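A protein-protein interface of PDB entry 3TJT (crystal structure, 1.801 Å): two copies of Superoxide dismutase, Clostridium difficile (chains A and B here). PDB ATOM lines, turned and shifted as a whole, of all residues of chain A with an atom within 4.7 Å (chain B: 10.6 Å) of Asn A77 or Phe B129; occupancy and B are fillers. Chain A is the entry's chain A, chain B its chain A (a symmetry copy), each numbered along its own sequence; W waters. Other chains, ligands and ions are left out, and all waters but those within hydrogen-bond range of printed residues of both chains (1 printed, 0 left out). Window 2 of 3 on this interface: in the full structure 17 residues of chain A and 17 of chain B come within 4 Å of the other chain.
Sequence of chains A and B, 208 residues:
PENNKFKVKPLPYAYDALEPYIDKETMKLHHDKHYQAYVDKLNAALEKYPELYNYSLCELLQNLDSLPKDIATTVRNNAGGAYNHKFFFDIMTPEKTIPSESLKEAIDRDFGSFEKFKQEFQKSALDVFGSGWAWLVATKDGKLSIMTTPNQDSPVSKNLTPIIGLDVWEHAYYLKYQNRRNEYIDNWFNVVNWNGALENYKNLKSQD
The side-chain hydroxyl (OH) of Tyr A38 lies within hydrogen-bond range of the side-chain amide nitrogen (NE2) of Gln A152 (2.9 Å).
The backbone carbonyl oxygen (O) of Asn A151 lies within hydrogen-bond range of the indole nitrogen (NE1) of Trp A169 (2.9 Å).
NE1 of Trp A169 lies close to NE2 of Gln A152, at 3.4 Å.
Among the printed residues, merely in contact across the chains: Tyr A38 with Phe B129 (3.8 Å), Asn A77 with Phe B129 (3.5 Å), Asn A151 with Phe B129 (3.9 Å), Asn A151 with Gly B130 (3.5 Å), Gln A152 with Phe B129 (3.7 Å), Trp A169 with Gly B130 (3.6 Å) and Trp A169 with Glu B170 (3.8 Å).
Of the printed residues of chain B, Asn A77 touches Phe B129.
Of chain A, only Tyr A38 (3.8 Å), Asn A77 (3.5 Å), Asn A151 (3.9 Å) and Gln A152 (3.7 Å) come within 4 Å of Phe B129.
No residue of chain B comes within 4 Å of Asn A78.
No residue of chain B comes within 4 Å of Gly A80.
No residue of chain B comes within 4 Å of Gly A81.
Asn A151 touches just these residues of chain B: Phe B129 and Gly B130.
Gln A152 touches just one residue of chain B: Phe B129.
Printed residues of chain B within 4 Å of Trp A169: Gly B130 and Glu B170.
Of the printed residues of chain B, Tyr A38 touches Phe B129.
Of the printed residues of chain A, Gly B130 touches Asn A151 (3.5 Å) and Trp A169 (3.6 Å).
Leu B126 touches none of the printed residues of chain A.
The nearest residue of chain B that does not touch Asn A77 is Asp B127 (7.0 Å).
The nearest residue of chain A that does not touch Phe B129 is Trp A169 (4.2 Å).
Of the 24 printed residues of chain B, 3 touch a printed residue of chain A.
Of the 13 printed residues of chain A, 5 touch a printed residue of chain B.
Hydrophobic or aromatic side chains of chain A that line the printed part of chain B: Tyr A38 and Trp A169.
Among the printed residues, 7 pairs touch across the chains.
Among the printed residues, no Asp or Glu carboxylate lies within 4 Å of a Lys or Arg side-chain nitrogen of the other chain.
Positions printed for both chains: 151, 152 and 169.
Of the 7 pairs that touch across the chains among the printed residues, none has its exchanged pair printed and touching as well.
Water W1 lies within hydrogen-bond range of OD1 of Asn B151 (2.9 Å), OD1 of Asn A151 (2.9 Å) and N of Ser B131 (3.0 Å).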
ATOM      1  N   TYR A  38      22.714   5.103 -12.428  1.00  0.00           N
ATOM      2  CA  TYR A  38      23.299   3.872 -11.880  1.00  0.00           C
ATOM      3  C   TYR A  38      22.368   3.227 -10.862  1.00  0.00           C
ATOM      4  O   TYR A  38      22.161   2.016 -10.871  1.00  0.00           O
ATOM      5  CB  TYR A  38      24.670   4.124 -11.253  1.00  0.00           C
ATOM      6  CG  TYR A  38      25.716   4.515 -12.267  1.00  0.00           C
ATOM      7  CD1 TYR A  38      26.012   3.685 -13.350  1.00  0.00           C
ATOM      8  CD2 TYR A  38      26.391   5.722 -12.157  1.00  0.00           C
ATOM      9  CE1 TYR A  38      26.969   4.055 -14.288  1.00  0.00           C
ATOM     10  CE2 TYR A  38      27.336   6.100 -13.088  1.00  0.00           C
ATOM     11  CZ  TYR A  38      27.624   5.257 -14.149  1.00  0.00           C
ATOM     12  OH  TYR A  38      28.570   5.647 -15.073  1.00  0.00           O
ATOM     13  N   THR A  73      27.231  -8.807 -14.641  1.00  0.00           N
ATOM     14  CA  THR A  73      27.835  -7.653 -15.298  1.00  0.00           C
ATOM     15  C   THR A  73      27.061  -6.370 -15.013  1.00  0.00           C
ATOM     16  O   THR A  73      27.656  -5.330 -14.729  1.00  0.00           O
ATOM     17  CB  THR A  73      27.959  -7.879 -16.819  1.00  0.00           C
ATOM     18  OG1 THR A  73      28.912  -8.919 -17.053  1.00  0.00           O
ATOM     19  CG2 THR A  73      28.434  -6.616 -17.518  1.00  0.00           C
ATOM     20  N   THR A  74      25.740  -6.436 -15.070  1.00  0.00           N
ATOM     21  CA  THR A  74      24.947  -5.235 -14.840  1.00  0.00           C
ATOM     22  C   THR A  74      25.113  -4.768 -13.396  1.00  0.00           C
ATOM     23  O   THR A  74      25.130  -3.570 -13.130  1.00  0.00           O
ATOM     24  CB  THR A  74      23.451  -5.424 -15.192  1.00  0.00           C
ATOM     25  OG1 THR A  74      22.753  -4.189 -14.992  1.00  0.00           O
ATOM     26  CG2 THR A  74      22.826  -6.484 -14.326  1.00  0.00           C
ATOM     27  N   VAL A  75      25.258  -5.707 -12.465  1.00  0.00           N
ATOM     28  CA  VAL A  75      25.517  -5.310 -11.081  1.00  0.00           C
ATOM     29  C   VAL A  75      26.914  -4.711 -10.920  1.00  0.00           C
ATOM     30  O   VAL A  75      27.083  -3.704 -10.240  1.00  0.00           O
ATOM     31  CB  VAL A  75      25.282  -6.460 -10.083  1.00  0.00           C
ATOM     32  CG1 VAL A  75      25.730  -6.039  -8.684  1.00  0.00           C
ATOM     33  CG2 VAL A  75      23.805  -6.855 -10.076  1.00  0.00           C
ATOM     34  N   ARG A  76      27.917  -5.316 -11.552  1.00  0.00           N
ATOM     35  CA  ARG A  76      29.267  -4.767 -11.522  1.00  0.00           C
ATOM     36  C   ARG A  76      29.244  -3.300 -11.960  1.00  0.00           C
ATOM     37  O   ARG A  76      29.782  -2.417 -11.292  1.00  0.00           O
ATOM     38  CB  ARG A  76      30.169  -5.576 -12.459  1.00  0.00           C
ATOM     39  CG  ARG A  76      31.550  -5.001 -12.694  1.00  0.00           C
ATOM     40  CD  ARG A  76      32.293  -5.925 -13.678  1.00  0.00           C
ATOM     41  NE  ARG A  76      33.644  -5.477 -13.996  1.00  0.00           N
ATOM     42  CZ  ARG A  76      34.488  -6.177 -14.752  1.00  0.00           C
ATOM     43  NH1 ARG A  76      34.112  -7.352 -15.250  1.00  0.00           N
ATOM     44  NH2 ARG A  76      35.706  -5.715 -15.005  1.00  0.00           N
ATOM     45  N   ASN A  77      28.596  -3.034 -13.082  1.00  0.00           N
ATOM     46  CA  ASN A  77      28.603  -1.673 -13.615  1.00  0.00           C
ATOM     47  C   ASN A  77      27.768  -0.690 -12.801  1.00  0.00           C
ATOM     48  O   ASN A  77      28.199   0.437 -12.557  1.00  0.00           O
ATOM     49  CB  ASN A  77      28.131  -1.671 -15.069  1.00  0.00           C
ATOM     50  CG  ASN A  77      29.110  -2.362 -15.994  1.00  0.00           C
ATOM     51  OD1 ASN A  77      30.299  -2.476 -15.685  1.00  0.00           O
ATOM     52  ND2 ASN A  77      28.614  -2.820 -17.150  1.00  0.00           N
ATOM     53  N   ASN A  78      26.584  -1.114 -12.374  1.00  0.00           N
ATOM     54  CA  ASN A  78      25.642  -0.177 -11.771  1.00  0.00           C
ATOM     55  C   ASN A  78      25.766  -0.071 -10.252  1.00  0.00           C
ATOM     56  O   ASN A  78      25.659   1.020  -9.701  1.00  0.00           O
ATOM     57  CB  ASN A  78      24.221  -0.486 -12.234  1.00  0.00           C
ATOM     58  CG  ASN A  78      24.052  -0.259 -13.730  1.00  0.00           C
ATOM     59  OD1 ASN A  78      23.920  -1.204 -14.521  1.00  0.00           O
ATOM     60  ND2 ASN A  78      24.107   0.996 -14.127  1.00  0.00           N
ATOM     61  N   ALA A  79      26.009  -1.190  -9.571  1.00  0.00           N
ATOM     62  CA  ALA A  79      26.385  -1.103  -8.156  1.00  0.00           C
ATOM     63  C   ALA A  79      27.718  -0.378  -8.055  1.00  0.00           C
ATOM     64  O   ALA A  79      27.946   0.385  -7.127  1.00  0.00           O
ATOM     65  CB  ALA A  79      26.472  -2.493  -7.501  1.00  0.00           C
ATOM     66  N   GLY A  80      28.603  -0.622  -9.019  1.00  0.00           N
ATOM     67  CA  GLY A  80      29.857   0.106  -9.071  1.00  0.00           C
ATOM     68  C   GLY A  80      29.603   1.603  -9.160  1.00  0.00           C
ATOM     69  O   GLY A  80      30.160   2.391  -8.383  1.00  0.00           O
ATOM     70  N   GLY A  81      28.763   1.995 -10.113  1.00  0.00           N
ATOM     71  CA  GLY A  81      28.458   3.403 -10.323  1.00  0.00           C
ATOM     72  C   GLY A  81      27.830   4.021  -9.087  1.00  0.00           C
ATOM     73  O   GLY A  81      28.199   5.122  -8.673  1.00  0.00           O
ATOM     74  N   ASN A 151      36.257   2.221 -15.863  1.00  0.00           N
ATOM     75  CA  ASN A 151      34.803   2.278 -15.872  1.00  0.00           C
ATOM     76  C   ASN A 151      34.237   2.470 -14.463  1.00  0.00           C
ATOM     77  O   ASN A 151      34.607   3.438 -13.815  1.00  0.00           O
ATOM     78  CB  ASN A 151      34.237   1.071 -16.623  1.00  0.00           C
ATOM     79  CG  ASN A 151      34.804   0.982 -18.026  1.00  0.00           C
ATOM     80  OD1 ASN A 151      34.973   2.011 -18.684  1.00  0.00           O
ATOM     81  ND2 ASN A 151      35.144  -0.232 -18.477  1.00  0.00           N
ATOM     82  N   GLN A 152      33.357   1.592 -13.989  1.00  0.00           N
ATOM     83  CA  GLN A 152      32.902   1.721 -12.591  1.00  0.00           C
ATOM     84  C   GLN A 152      33.388   0.581 -11.708  1.00  0.00           C
ATOM     85  O   GLN A 152      32.782   0.284 -10.676  1.00  0.00           O
ATOM     86  CB  GLN A 152      31.382   1.846 -12.475  1.00  0.00           C
ATOM     87  CG  GLN A 152      30.776   3.047 -13.230  1.00  0.00           C
ATOM     88  CD  GLN A 152      31.229   4.404 -12.703  1.00  0.00           C
ATOM     89  OE1 GLN A 152      31.790   4.508 -11.590  1.00  0.00           O
ATOM     90  NE2 GLN A 152      30.995   5.445 -13.479  1.00  0.00           N
ATOM     91  N   TRP A 169      36.190  10.012 -15.440  1.00  0.00           N
ATOM     92  CA  TRP A 169      35.297   9.938 -16.594  1.00  0.00           C
ATOM     93  C   TRP A 169      35.203  11.357 -17.126  1.00  0.00           C
ATOM     94  O   TRP A 169      35.231  12.323 -16.351  1.00  0.00           O
ATOM     95  CB  TRP A 169      33.900   9.486 -16.188  1.00  0.00           C
ATOM     96  CG  TRP A 169      33.739   8.006 -15.941  1.00  0.00           C
ATOM     97  CD1 TRP A 169      34.434   7.236 -15.044  1.00  0.00           C
ATOM     98  CD2 TRP A 169      32.802   7.134 -16.579  1.00  0.00           C
ATOM     99  NE1 TRP A 169      33.984   5.934 -15.094  1.00  0.00           N
ATOM    100  CE2 TRP A 169      32.977   5.846 -16.020  1.00  0.00           C
ATOM    101  CE3 TRP A 169      31.825   7.314 -17.564  1.00  0.00           C
ATOM    102  CZ2 TRP A 169      32.215   4.746 -16.422  1.00  0.00           C
ATOM    103  CZ3 TRP A 169      31.056   6.215 -17.961  1.00  0.00           C
ATOM    104  CH2 TRP A 169      31.259   4.948 -17.390  1.00  0.00           C
ATOM    105  N   GLN B 122      21.950   2.119 -33.307  1.00  0.00           N
ATOM    106  CA  GLN B 122      21.669   3.089 -32.253  1.00  0.00           C
ATOM    107  C   GLN B 122      21.695   2.447 -30.870  1.00  0.00           C
ATOM    108  O   GLN B 122      22.241   3.019 -29.933  1.00  0.00           O
ATOM    109  CB  GLN B 122      20.345   3.809 -32.496  1.00  0.00           C
ATOM    110  CG  GLN B 122      20.380   4.700 -33.721  1.00  0.00           C
ATOM    111  CD  GLN B 122      19.371   5.836 -33.640  1.00  0.00           C
ATOM    112  OE1 GLN B 122      18.848   6.292 -34.654  1.00  0.00           O
ATOM    113  NE2 GLN B 122      19.105   6.304 -32.428  1.00  0.00           N
ATOM    114  N   LYS B 123      21.123   1.256 -30.748  1.00  0.00           N
ATOM    115  CA  LYS B 123      21.132   0.548 -29.470  1.00  0.00           C
ATOM    116  C   LYS B 123      22.542   0.131 -29.052  1.00  0.00           C
ATOM    117  O   LYS B 123      22.910   0.239 -27.875  1.00  0.00           O
ATOM    118  CB  LYS B 123      20.223  -0.679 -29.515  1.00  0.00           C
ATOM    119  CG  LYS B 123      20.053  -1.335 -28.150  1.00  0.00           C
ATOM    120  CD  LYS B 123      19.059  -2.477 -28.206  1.00  0.00           C
ATOM    121  CE  LYS B 123      18.540  -2.818 -26.811  1.00  0.00           C
ATOM    122  NZ  LYS B 123      19.633  -3.168 -25.858  1.00  0.00           N
ATOM    123  N   SER B 124      23.328  -0.357 -30.005  1.00  0.00           N
ATOM    124  CA  SER B 124      24.703  -0.741 -29.696  1.00  0.00           C
ATOM    125  C   SER B 124      25.511   0.460 -29.228  1.00  0.00           C
ATOM    126  O   SER B 124      26.277   0.362 -28.267  1.00  0.00           O
ATOM    127  CB  SER B 124      25.385  -1.414 -30.894  1.00  0.00           C
ATOM    128  OG  SER B 124      24.784  -2.674 -31.168  1.00  0.00           O
ATOM    129  N   ALA B 125      25.333   1.592 -29.908  1.00  0.00           N
ATOM    130  CA  ALA B 125      26.017   2.827 -29.531  1.00  0.00           C
ATOM    131  C   ALA B 125      25.588   3.292 -28.134  1.00  0.00           C
ATOM    132  O   ALA B 125      26.414   3.754 -27.330  1.00  0.00           O
ATOM    133  CB  ALA B 125      25.732   3.923 -30.562  1.00  0.00           C
ATOM    134  N   LEU B 126      24.297   3.172 -27.850  1.00  0.00           N
ATOM    135  CA  LEU B 126      23.766   3.621 -26.565  1.00  0.00           C
ATOM    136  C   LEU B 126      24.277   2.759 -25.421  1.00  0.00           C
ATOM    137  O   LEU B 126      24.490   3.247 -24.313  1.00  0.00           O
ATOM    138  CB  LEU B 126      22.238   3.598 -26.584  1.00  0.00           C
ATOM    139  CG  LEU B 126      21.557   4.202 -25.352  1.00  0.00           C
ATOM    140  CD1 LEU B 126      21.753   5.710 -25.350  1.00  0.00           C
ATOM    141  CD2 LEU B 126      20.072   3.834 -25.311  1.00  0.00           C
ATOM    142  N   ASP B 127      24.480   1.476 -25.697  1.00  0.00           N
ATOM    143  CA  ASP B 127      24.827   0.517 -24.652  1.00  0.00           C
ATOM    144  C   ASP B 127      26.330   0.393 -24.353  1.00  0.00           C
ATOM    145  O   ASP B 127      26.716  -0.310 -23.418  1.00  0.00           O
ATOM    146  CB  ASP B 127      24.241  -0.863 -24.979  1.00  0.00           C
ATOM    147  CG  ASP B 127      22.721  -0.910 -24.850  1.00  0.00           C
ATOM    148  OD1 ASP B 127      22.111   0.070 -24.368  1.00  0.00           O
ATOM    149  OD2 ASP B 127      22.128  -1.940 -25.237  1.00  0.00           O
ATOM    150  N   VAL B 128      27.185   1.063 -25.124  1.00  0.00           N
ATOM    151  CA  VAL B 128      28.607   1.045 -24.820  1.00  0.00           C
ATOM    152  C   VAL B 128      28.791   1.602 -23.417  1.00  0.00           C
ATOM    153  O   VAL B 128      28.322   2.708 -23.115  1.00  0.00           O
ATOM    154  CB  VAL B 128      29.435   1.893 -25.811  1.00  0.00           C
ATOM    155  CG1 VAL B 128      30.848   2.086 -25.292  1.00  0.00           C
ATOM    156  CG2 VAL B 128      29.450   1.233 -27.201  1.00  0.00           C
ATOM    157  N   PHE B 129      29.441   0.828 -22.551  1.00  0.00           N
ATOM    158  CA  PHE B 129      29.638   1.254 -21.168  1.00  0.00           C
ATOM    159  C   PHE B 129      31.052   1.763 -20.968  1.00  0.00           C
ATOM    160  O   PHE B 129      32.022   1.028 -21.169  1.00  0.00           O
ATOM    161  CB  PHE B 129      29.356   0.119 -20.179  1.00  0.00           C
ATOM    162  CG  PHE B 129      29.285   0.587 -18.758  1.00  0.00           C
ATOM    163  CD1 PHE B 129      28.125   1.176 -18.279  1.00  0.00           C
ATOM    164  CD2 PHE B 129      30.382   0.484 -17.919  1.00  0.00           C
ATOM    165  CE1 PHE B 129      28.052   1.640 -16.961  1.00  0.00           C
ATOM    166  CE2 PHE B 129      30.322   0.938 -16.598  1.00  0.00           C
ATOM    167  CZ  PHE B 129      29.159   1.523 -16.126  1.00  0.00           C
ATOM    168  N   GLY B 130      31.170   3.024 -20.562  1.00  0.00           N
ATOM    169  CA  GLY B 130      32.463   3.664 -20.498  1.00  0.00           C
ATOM    170  C   GLY B 130      32.746   4.316 -21.841  1.00  0.00           C
ATOM    171  O   GLY B 130      31.810   4.718 -22.543  1.00  0.00           O
ATOM    172  N   SER B 131      34.022   4.405 -22.190  1.00  0.00           N
ATOM    173  CA  SER B 131      34.470   5.028 -23.442  1.00  0.00           C
ATOM    174  C   SER B 131      34.532   3.988 -24.547  1.00  0.00           C
ATOM    175  O   SER B 131      34.921   2.841 -24.306  1.00  0.00           O
ATOM    176  CB  SER B 131      35.867   5.634 -23.273  1.00  0.00           C
ATOM    177  OG  SER B 131      35.897   6.634 -22.244  1.00  0.00           O
ATOM    178  N   GLY B 132      34.166   4.373 -25.766  1.00  0.00           N
ATOM    179  CA  GLY B 132      34.336   3.449 -26.878  1.00  0.00           C
ATOM    180  C   GLY B 132      33.643   3.893 -28.146  1.00  0.00           C
ATOM    181  O   GLY B 132      33.339   5.070 -28.307  1.00  0.00           O
ATOM    182  N   TRP B 133      33.402   2.931 -29.037  1.00  0.00           N
ATOM    183  CA  TRP B 133      32.948   3.190 -30.408  1.00  0.00           C
ATOM    184  C   TRP B 133      31.905   2.156 -30.804  1.00  0.00           C
ATOM    185  O   TRP B 133      31.959   1.009 -30.356  1.00  0.00           O
ATOM    186  CB  TRP B 133      34.128   3.058 -31.381  1.00  0.00           C
ATOM    187  CG  TRP B 133      35.169   4.104 -31.227  1.00  0.00           C
ATOM    188  CD1 TRP B 133      36.131   4.169 -30.260  1.00  0.00           C
ATOM    189  CD2 TRP B 133      35.369   5.244 -32.070  1.00  0.00           C
ATOM    190  NE1 TRP B 133      36.908   5.283 -30.443  1.00  0.00           N
ATOM    191  CE2 TRP B 133      36.463   5.961 -31.549  1.00  0.00           C
ATOM    192  CE3 TRP B 133      34.734   5.720 -33.222  1.00  0.00           C
ATOM    193  CZ2 TRP B 133      36.938   7.136 -32.131  1.00  0.00           C
ATOM    194  CZ3 TRP B 133      35.208   6.893 -33.807  1.00  0.00           C
ATOM    195  CH2 TRP B 133      36.297   7.586 -33.259  1.00  0.00           C
ATOM    196  N   ALA B 134      30.958   2.550 -31.655  1.00  0.00           N
ATOM    197  CA  ALA B 134      30.072   1.580 -32.300  1.00  0.00           C
ATOM    198  C   ALA B 134      30.410   1.547 -33.784  1.00  0.00           C
ATOM    199  O   ALA B 134      30.655   2.591 -34.383  1.00  0.00           O
ATOM    200  CB  ALA B 134      28.611   1.952 -32.104  1.00  0.00           C
ATOM    201  N   THR B 148      30.918  -3.271 -31.161  1.00  0.00           N
ATOM    202  CA  THR B 148      31.513  -2.138 -30.459  1.00  0.00           C
ATOM    203  C   THR B 148      32.940  -2.460 -30.024  1.00  0.00           C
ATOM    204  O   THR B 148      33.335  -3.630 -29.945  1.00  0.00           O
ATOM    205  CB  THR B 148      30.677  -1.729 -29.230  1.00  0.00           C
ATOM    206  OG1 THR B 148      30.695  -2.791 -28.265  1.00  0.00           O
ATOM    207  CG2 THR B 148      29.248  -1.452 -29.638  1.00  0.00           C
ATOM    208  N   THR B 149      33.723  -1.419 -29.777  1.00  0.00           N
ATOM    209  CA  THR B 149      35.051  -1.576 -29.196  1.00  0.00           C
ATOM    210  C   THR B 149      35.203  -0.616 -28.020  1.00  0.00           C
ATOM    211  O   THR B 149      34.614   0.474 -28.018  1.00  0.00           O
ATOM    212  CB  THR B 149      36.188  -1.282 -30.198  1.00  0.00           C
ATOM    213  OG1 THR B 149      36.042   0.052 -30.715  1.00  0.00           O
ATOM    214  CG2 THR B 149      36.200  -2.302 -31.358  1.00  0.00           C
ATOM    215  N   PRO B 150      35.990  -1.014 -27.011  1.00  0.00           N
ATOM    216  CA  PRO B 150      36.247  -0.107 -25.884  1.00  0.00           C
ATOM    217  C   PRO B 150      37.411   0.827 -26.155  1.00  0.00           C
ATOM    218  O   PRO B 150      38.325   0.482 -26.903  1.00  0.00           O
ATOM    219  CB  PRO B 150      36.647  -1.069 -24.761  1.00  0.00           C
ATOM    220  CG  PRO B 150      37.340  -2.201 -25.498  1.00  0.00           C
ATOM    221  CD  PRO B 150      36.597  -2.349 -26.810  1.00  0.00           C
ATOM    222  N   ASN B 151      37.391   1.999 -25.522  1.00  0.00           N
ATOM    223  CA  ASN B 151      38.526   2.908 -25.572  1.00  0.00           C
ATOM    224  C   ASN B 151      38.918   3.241 -27.013  1.00  0.00           C
ATOM    225  O   ASN B 151      38.070   3.721 -27.750  1.00  0.00           O
ATOM    226  CB  ASN B 151      39.670   2.365 -24.713  1.00  0.00           C
ATOM    227  CG  ASN B 151      39.215   2.113 -23.288  1.00  0.00           C
ATOM    228  OD1 ASN B 151      38.444   2.906 -22.743  1.00  0.00           O
ATOM    229  ND2 ASN B 151      39.645   0.994 -22.693  1.00  0.00           N
ATOM    230  N   GLN B 152      40.165   3.010 -27.419  1.00  0.00           N
ATOM    231  CA  GLN B 152      40.504   3.228 -28.839  1.00  0.00           C
ATOM    232  C   GLN B 152      40.823   1.932 -29.571  1.00  0.00           C
ATOM    233  O   GLN B 152      41.524   1.941 -30.585  1.00  0.00           O
ATOM    234  CB  GLN B 152      41.658   4.216 -29.023  1.00  0.00           C
ATOM    235  CG  GLN B 152      41.404   5.618 -28.428  1.00  0.00           C
ATOM    236  CD  GLN B 152      40.254   6.373 -29.085  1.00  0.00           C
ATOM    237  OE1 GLN B 152      39.782   5.999 -30.181  1.00  0.00           O
ATOM    238  NE2 GLN B 152      39.797   7.427 -28.439  1.00  0.00           N
ATOM    239  N   VAL B 168      31.662   7.317 -29.138  1.00  0.00           N
ATOM    240  CA  VAL B 168      30.795   7.606 -27.990  1.00  0.00           C
ATOM    241  C   VAL B 168      31.562   7.854 -26.692  1.00  0.00           C
ATOM    242  O   VAL B 168      30.996   7.737 -25.603  1.00  0.00           O
ATOM    243  CB  VAL B 168      29.657   6.556 -27.774  1.00  0.00           C
ATOM    244  CG1 VAL B 168      28.646   6.612 -28.917  1.00  0.00           C
ATOM    245  CG2 VAL B 168      30.220   5.145 -27.618  1.00  0.00           C
ATOM    246  N   TRP B 169      32.838   8.204 -26.808  1.00  0.00           N
ATOM    247  CA  TRP B 169      33.557   8.803 -25.685  1.00  0.00           C
ATOM    248  C   TRP B 169      32.772  10.049 -25.318  1.00  0.00           C
ATOM    249  O   TRP B 169      32.205  10.716 -26.194  1.00  0.00           O
ATOM    250  CB  TRP B 169      34.964   9.226 -26.090  1.00  0.00           C
ATOM    251  CG  TRP B 169      35.980   8.114 -26.176  1.00  0.00           C
ATOM    252  CD1 TRP B 169      35.912   6.988 -26.957  1.00  0.00           C
ATOM    253  CD2 TRP B 169      37.228   8.045 -25.481  1.00  0.00           C
ATOM    254  NE1 TRP B 169      37.044   6.222 -26.780  1.00  0.00           N
ATOM    255  CE2 TRP B 169      37.871   6.853 -25.888  1.00  0.00           C
ATOM    256  CE3 TRP B 169      37.871   8.877 -24.559  1.00  0.00           C
ATOM    257  CZ2 TRP B 169      39.123   6.472 -25.394  1.00  0.00           C
ATOM    258  CZ3 TRP B 169      39.126   8.502 -24.070  1.00  0.00           C
ATOM    259  CH2 TRP B 169      39.736   7.308 -24.490  1.00  0.00           C
ATOM    260  N   GLU B 170      32.747  10.392 -24.037  1.00  0.00           N
ATOM    261  CA  GLU B 170      31.990  11.569 -23.636  1.00  0.00           C
ATOM    262  C   GLU B 170      32.530  12.873 -24.237  1.00  0.00           C
ATOM    263  O   GLU B 170      31.756  13.810 -24.452  1.00  0.00           O
ATOM    264  CB  GLU B 170      31.853  11.624 -22.106  1.00  0.00           C
ATOM    265  CG  GLU B 170      30.865  10.572 -21.606  1.00  0.00           C
ATOM    266  CD  GLU B 170      30.867  10.391 -20.092  1.00  0.00           C
ATOM    267  OE1 GLU B 170      31.932  10.562 -19.455  1.00  0.00           O
ATOM    268  OE2 GLU B 170      29.789  10.074 -19.558  1.00  0.00           O
ATOM    269  N   TYR B 173      30.502  14.311 -27.246  1.00  0.00           N
ATOM    270  CA  TYR B 173      29.133  14.795 -27.179  1.00  0.00           C
ATOM    271  C   TYR B 173      28.749  15.599 -25.934  1.00  0.00           C
ATOM    272  O   TYR B 173      27.643  16.128 -25.881  1.00  0.00           O
ATOM    273  CB  TYR B 173      28.129  13.648 -27.361  1.00  0.00           C
ATOM    274  CG  TYR B 173      28.121  12.574 -26.275  1.00  0.00           C
ATOM    275  CD1 TYR B 173      27.377  12.734 -25.103  1.00  0.00           C
ATOM    276  CD2 TYR B 173      28.823  11.383 -26.448  1.00  0.00           C
ATOM    277  CE1 TYR B 173      27.344  11.718 -24.117  1.00  0.00           C
ATOM    278  CE2 TYR B 173      28.801  10.373 -25.468  1.00  0.00           C
ATOM    279  CZ  TYR B 173      28.066  10.547 -24.316  1.00  0.00           C
ATOM    280  OH  TYR B 173      28.046   9.543 -23.362  1.00  0.00           O
ATOM    281  N   ARG B 181      23.253  10.865 -24.391  1.00  0.00           N
ATOM    282  CA  ARG B 181      23.939  10.238 -25.516  1.00  0.00           C
ATOM    283  C   ARG B 181      22.953   9.813 -26.609  1.00  0.00           C
ATOM    284  O   ARG B 181      23.266   9.867 -27.803  1.00  0.00           O
ATOM    285  CB  ARG B 181      24.788   9.043 -25.054  1.00  0.00           C
ATOM    286  CG  ARG B 181      25.706   8.511 -26.163  1.00  0.00           C
ATOM    287  CD  ARG B 181      26.190   7.079 -25.869  1.00  0.00           C
ATOM    288  NE  ARG B 181      27.111   7.036 -24.740  1.00  0.00           N
ATOM    289  CZ  ARG B 181      27.636   5.911 -24.256  1.00  0.00           C
ATOM    290  NH1 ARG B 181      27.343   4.743 -24.819  1.00  0.00           N
ATOM    291  NH2 ARG B 181      28.459   5.954 -23.215  1.00  0.00           N
ATOM    292  N   ILE B 185      23.400  10.337 -30.656  1.00  0.00           N
ATOM    293  CA  ILE B 185      23.391   9.218 -31.599  1.00  0.00           C
ATOM    294  C   ILE B 185      22.363   9.449 -32.703  1.00  0.00           C
ATOM    295  O   ILE B 185      22.662   9.318 -33.892  1.00  0.00           O
ATOM    296  CB  ILE B 185      23.106   7.885 -30.882  1.00  0.00           C
ATOM    297  CG1 ILE B 185      24.247   7.574 -29.906  1.00  0.00           C
ATOM    298  CG2 ILE B 185      22.925   6.763 -31.901  1.00  0.00           C
ATOM    299  CD1 ILE B 185      23.890   6.532 -28.844  1.00  0.00           C
HETATM  300  O   HOH W   1      36.419   3.337 -20.768  1.00  0.00           O
